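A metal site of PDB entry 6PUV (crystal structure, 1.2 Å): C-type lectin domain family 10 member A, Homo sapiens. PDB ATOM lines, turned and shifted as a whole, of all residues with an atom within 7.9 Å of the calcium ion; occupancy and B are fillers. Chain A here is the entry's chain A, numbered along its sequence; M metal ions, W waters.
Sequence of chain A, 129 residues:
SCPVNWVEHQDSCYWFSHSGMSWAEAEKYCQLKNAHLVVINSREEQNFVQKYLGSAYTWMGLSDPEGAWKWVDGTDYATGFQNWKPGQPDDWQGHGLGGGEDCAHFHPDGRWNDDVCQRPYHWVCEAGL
The calcium ion is bound by O of Val 39, OD1 of Asn 41, water W1, OE2 of Glu 45, water W2, OE2 of Glu 126, OE1 of Glu 45 and OE1 of Glu 126.
OE2 of Glu 126 lies close to OG of Ser 12 (2.7 Å). The side-chain carboxylate (OE2) of Glu 45 lies close to the side-chain hydroxyl (OH) of Tyr 14. The backbone carbonyl oxygen of His 36 sits at hydrogen-bond distance from the backbone NH of Glu 126, at 2.8 Å. The side-chain hydroxyl (OG) of Ser 42 lies within hydrogen-bond range of the backbone NH (N) of Glu 45.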
ATOM      1  N   SER A  12     -20.506  16.706  -4.655  1.00  0.00           N
ATOM      2  CA  SER A  12     -20.902  17.833  -5.484  1.00  0.00           C
ATOM      3  C   SER A  12     -21.692  18.830  -4.656  1.00  0.00           C
ATOM      4  O   SER A  12     -22.358  18.483  -3.699  1.00  0.00           O
ATOM      5  CB  SER A  12     -21.706  17.408  -6.660  1.00  0.00           C
ATOM      6  OG  SER A  12     -20.885  16.817  -7.651  1.00  0.00           O
ATOM      7  N   TYR A  14     -24.624  21.841  -5.608  1.00  0.00           N
ATOM      8  CA  TYR A  14     -25.599  22.189  -6.668  1.00  0.00           C
ATOM      9  C   TYR A  14     -26.278  23.499  -6.334  1.00  0.00           C
ATOM     10  O   TYR A  14     -26.651  23.747  -5.208  1.00  0.00           O
ATOM     11  CB  TYR A  14     -26.665  21.108  -6.841  1.00  0.00           C
ATOM     12  CG  TYR A  14     -26.070  19.732  -7.119  1.00  0.00           C
ATOM     13  CD1 TYR A  14     -25.665  18.922  -6.078  1.00  0.00           C
ATOM     14  CD2 TYR A  14     -25.924  19.262  -8.414  1.00  0.00           C
ATOM     15  CE1 TYR A  14     -25.148  17.654  -6.325  1.00  0.00           C
ATOM     16  CE2 TYR A  14     -25.396  18.014  -8.685  1.00  0.00           C
ATOM     17  CZ  TYR A  14     -25.039  17.205  -7.627  1.00  0.00           C
ATOM     18  OH  TYR A  14     -24.493  15.967  -7.818  1.00  0.00           O
ATOM     19  N   HIS A  36     -20.188  24.037 -13.576  1.00  0.00           N
ATOM     20  CA  HIS A  36     -20.706  23.760 -14.925  1.00  0.00           C
ATOM     21  C   HIS A  36     -22.178  23.452 -14.818  1.00  0.00           C
ATOM     22  O   HIS A  36     -22.642  23.050 -13.753  1.00  0.00           O
ATOM     23  CB  HIS A  36     -19.960  22.573 -15.549  1.00  0.00           C
ATOM     24  CG  HIS A  36     -19.868  21.364 -14.668  1.00  0.00           C
ATOM     25  ND1 HIS A  36     -20.902  20.450 -14.601  1.00  0.00           N
ATOM     26  CD2 HIS A  36     -18.892  20.889 -13.842  1.00  0.00           C
ATOM     27  CE1 HIS A  36     -20.613  19.485 -13.741  1.00  0.00           C
ATOM     28  NE2 HIS A  36     -19.340  19.716 -13.292  1.00  0.00           N
ATOM     29  N   LEU A  37     -22.855  23.523 -15.930  1.00  0.00           N
ATOM     30  CA  LEU A  37     -24.233  23.043 -15.970  1.00  0.00           C
ATOM     31  C   LEU A  37     -24.221  21.595 -15.509  1.00  0.00           C
ATOM     32  O   LEU A  37     -23.288  20.826 -15.902  1.00  0.00           O
ATOM     33  CB  LEU A  37     -24.815  23.129 -17.373  1.00  0.00           C
ATOM     34  CG  LEU A  37     -25.320  24.503 -17.796  1.00  0.00           C
ATOM     35  CD1 LEU A  37     -25.675  24.512 -19.273  1.00  0.00           C
ATOM     36  CD2 LEU A  37     -26.528  24.893 -16.972  1.00  0.00           C
ATOM     37  N   VAL A  38     -25.204  21.156 -14.765  1.00  0.00           N
ATOM     38  CA  VAL A  38     -25.168  19.855 -14.077  1.00  0.00           C
ATOM     39  C   VAL A  38     -24.952  18.746 -15.097  1.00  0.00           C
ATOM     40  O   VAL A  38     -25.582  18.666 -16.144  1.00  0.00           O
ATOM     41  CB  VAL A  38     -26.428  19.650 -13.235  1.00  0.00           C
ATOM     42  CG1 VAL A  38     -27.717  19.596 -14.055  1.00  0.00           C
ATOM     43  CG2 VAL A  38     -26.336  18.443 -12.332  1.00  0.00           C
ATOM     44  N   VAL A  39     -24.096  17.800 -14.698  1.00  0.00           N
ATOM     45  CA  VAL A  39     -23.878  16.533 -15.451  1.00  0.00           C
ATOM     46  C   VAL A  39     -24.401  15.391 -14.592  1.00  0.00           C
ATOM     47  O   VAL A  39     -23.976  15.281 -13.429  1.00  0.00           O
ATOM     48  CB  VAL A  39     -22.385  16.365 -15.785  1.00  0.00           C
ATOM     49  CG1 VAL A  39     -22.094  15.003 -16.391  1.00  0.00           C
ATOM     50  CG2 VAL A  39     -21.919  17.481 -16.694  1.00  0.00           C
ATOM     51  N   ILE A  40     -25.391  14.671 -15.106  1.00  0.00           N
ATOM     52  CA  ILE A  40     -26.039  13.598 -14.331  1.00  0.00           C
ATOM     53  C   ILE A  40     -25.272  12.303 -14.623  1.00  0.00           C
ATOM     54  O   ILE A  40     -25.393  11.767 -15.728  1.00  0.00           O
ATOM     55  CB  ILE A  40     -27.518  13.456 -14.639  1.00  0.00           C
ATOM     56  CG1 ILE A  40     -28.279  14.775 -14.437  1.00  0.00           C
ATOM     57  CG2 ILE A  40     -28.116  12.325 -13.813  1.00  0.00           C
ATOM     58  CD1 ILE A  40     -28.299  15.261 -13.001  1.00  0.00           C
ATOM     59  N   ASN A  41     -24.491  11.821 -13.645  1.00  0.00           N
ATOM     60  CA  ASN A  41     -23.569  10.679 -13.828  1.00  0.00           C
ATOM     61  C   ASN A  41     -24.207   9.373 -13.395  1.00  0.00           C
ATOM     62  O   ASN A  41     -23.589   8.312 -13.613  1.00  0.00           O
ATOM     63  CB  ASN A  41     -22.298  10.941 -13.027  1.00  0.00           C
ATOM     64  CG  ASN A  41     -21.557  12.171 -13.524  1.00  0.00           C
ATOM     65  OD1 ASN A  41     -21.801  13.273 -13.024  1.00  0.00           O
ATOM     66  ND2 ASN A  41     -20.650  12.012 -14.479  1.00  0.00           N
ATOM     67  N   SER A  42     -25.344   9.392 -12.686  1.00  0.00           N
ATOM     68  CA  SER A  42     -25.889   8.170 -12.059  1.00  0.00           C
ATOM     69  C   SER A  42     -27.351   8.365 -11.713  1.00  0.00           C
ATOM     70  O   SER A  42     -27.780   9.511 -11.607  1.00  0.00           O
ATOM     71  CB  SER A  42     -25.099   7.827 -10.799  1.00  0.00           C
ATOM     72  OG  SER A  42     -25.325   8.797  -9.765  1.00  0.00           O
ATOM     73  N   GLU A  45     -27.614  10.358  -8.406  1.00  0.00           N
ATOM     74  CA  GLU A  45     -27.449  11.791  -8.663  1.00  0.00           C
ATOM     75  C   GLU A  45     -28.742  12.344  -9.293  1.00  0.00           C
ATOM     76  O   GLU A  45     -29.242  13.421  -8.839  1.00  0.00           O
ATOM     77  CB  GLU A  45     -26.252  12.084  -9.540  1.00  0.00           C
ATOM     78  CG  GLU A  45     -26.111  13.584  -9.713  1.00  0.00           C
ATOM     79  CD  GLU A  45     -24.847  14.002 -10.426  1.00  0.00           C
ATOM     80  OE1 GLU A  45     -24.303  13.220 -11.217  1.00  0.00           O
ATOM     81  OE2 GLU A  45     -24.433  15.202 -10.225  1.00  0.00           O
ATOM     82  N   GLN A  46     -29.298  11.648 -10.268  1.00  0.00           N
ATOM     83  CA  GLN A  46     -30.610  12.016 -10.863  1.00  0.00           C
ATOM     84  C   GLN A  46     -31.637  12.205  -9.751  1.00  0.00           C
ATOM     85  O   GLN A  46     -32.395  13.167  -9.749  1.00  0.00           O
ATOM     86  CB  GLN A  46     -31.051  10.930 -11.848  1.00  0.00           C
ATOM     87  CG  GLN A  46     -32.472  11.144 -12.399  1.00  0.00           C
ATOM     88  CD  GLN A  46     -32.654  12.355 -13.282  1.00  0.00           C
ATOM     89  OE1 GLN A  46     -31.803  12.605 -14.142  1.00  0.00           O
ATOM     90  NE2 GLN A  46     -33.736  13.101 -13.054  1.00  0.00           N
ATOM     91  N   VAL A  49     -30.947  15.415  -7.602  1.00  0.00           N
ATOM     92  CA  VAL A  49     -31.102  16.690  -8.328  1.00  0.00           C
ATOM     93  C   VAL A  49     -32.601  16.904  -8.589  1.00  0.00           C
ATOM     94  O   VAL A  49     -33.135  18.031  -8.427  1.00  0.00           O
ATOM     95  CB  VAL A  49     -30.295  16.691  -9.629  1.00  0.00           C
ATOM     96  CG1 VAL A  49     -30.674  17.850 -10.546  1.00  0.00           C
ATOM     97  CG2 VAL A  49     -28.819  16.713  -9.318  1.00  0.00           C
ATOM     98  N   TRP A  71     -21.944  15.698 -23.046  1.00  0.00           N
ATOM     99  CA  TRP A  71     -21.925  16.376 -21.734  1.00  0.00           C
ATOM    100  C   TRP A  71     -20.874  17.479 -21.769  1.00  0.00           C
ATOM    101  O   TRP A  71     -19.768  17.275 -22.335  1.00  0.00           O
ATOM    102  CB  TRP A  71     -21.668  15.383 -20.613  1.00  0.00           C
ATOM    103  CG  TRP A  71     -22.769  14.415 -20.364  1.00  0.00           C
ATOM    104  CD1 TRP A  71     -22.796  13.119 -20.745  1.00  0.00           C
ATOM    105  CD2 TRP A  71     -24.026  14.670 -19.707  1.00  0.00           C
ATOM    106  NE1 TRP A  71     -23.957  12.526 -20.317  1.00  0.00           N
ATOM    107  CE2 TRP A  71     -24.714  13.443 -19.662  1.00  0.00           C
ATOM    108  CE3 TRP A  71     -24.575  15.764 -19.049  1.00  0.00           C
ATOM    109  CZ2 TRP A  71     -25.943  13.283 -19.042  1.00  0.00           C
ATOM    110  CZ3 TRP A  71     -25.828  15.645 -18.482  1.00  0.00           C
ATOM    111  CH2 TRP A  71     -26.518  14.424 -18.496  1.00  0.00           C
ATOM    112  N   ASP A  73     -18.749  18.560 -19.685  1.00  0.00           N
ATOM    113  CA  ASP A  73     -17.445  18.322 -19.037  1.00  0.00           C
ATOM    114  C   ASP A  73     -16.707  17.162 -19.725  1.00  0.00           C
ATOM    115  O   ASP A  73     -15.664  16.755 -19.211  1.00  0.00           O
ATOM    116  CB  ASP A  73     -17.623  18.084 -17.549  1.00  0.00           C
ATOM    117  CG  ASP A  73     -18.271  16.757 -17.241  1.00  0.00           C
ATOM    118  OD1 ASP A  73     -18.820  16.150 -18.186  1.00  0.00           O
ATOM    119  OD2 ASP A  73     -18.211  16.350 -16.090  1.00  0.00           O
ATOM    120  N   THR A  75     -17.845  14.064 -20.100  1.00  0.00           N
ATOM    121  CA  THR A  75     -18.390  12.759 -19.655  1.00  0.00           C
ATOM    122  C   THR A  75     -18.951  11.998 -20.864  1.00  0.00           C
ATOM    123  O   THR A  75     -19.669  12.612 -21.702  1.00  0.00           O
ATOM    124  CB  THR A  75     -19.473  12.922 -18.593  1.00  0.00           C
ATOM    125  OG1 THR A  75     -18.878  13.496 -17.446  1.00  0.00           O
ATOM    126  CG2 THR A  75     -20.156  11.626 -18.215  1.00  0.00           C
ATOM    127  N   GLU A 126     -23.355  22.757 -11.074  1.00  0.00           N
ATOM    128  CA  GLU A 126     -22.707  21.686 -10.255  1.00  0.00           C
ATOM    129  C   GLU A 126     -21.231  22.045 -10.146  1.00  0.00           C
ATOM    130  O   GLU A 126     -20.569  22.277 -11.159  1.00  0.00           O
ATOM    131  CB  GLU A 126     -22.918  20.338 -10.924  1.00  0.00           C
ATOM    132  CG  GLU A 126     -22.229  19.217 -10.168  1.00  0.00           C
ATOM    133  CD  GLU A 126     -22.364  17.859 -10.804  1.00  0.00           C
ATOM    134  OE1 GLU A 126     -22.822  17.733 -11.928  1.00  0.00           O
ATOM    135  OE2 GLU A 126     -21.930  16.882 -10.127  1.00  0.00           O
ATOM    136  N   ALA A 127     -20.743  22.007  -8.933  1.00  0.00           N
ATOM    137  CA  ALA A 127     -19.332  22.251  -8.608  1.00  0.00           C
ATOM    138  C   ALA A 127     -18.824  21.136  -7.686  1.00  0.00           C
ATOM    139  O   ALA A 127     -19.590  20.465  -7.041  1.00  0.00           O
ATOM    140  CB  ALA A 127     -19.118  23.574  -7.941  1.00  0.00           C
HETATM  141 CA    CA M   1     -22.483  15.069 -11.679  1.00  0.00          CA
HETATM  142  O   HOH W   1     -20.444  15.823 -12.623  1.00  0.00           O
HETATM  143  O   HOH W   2     -21.306  13.739  -9.994  1.00  0.00           O
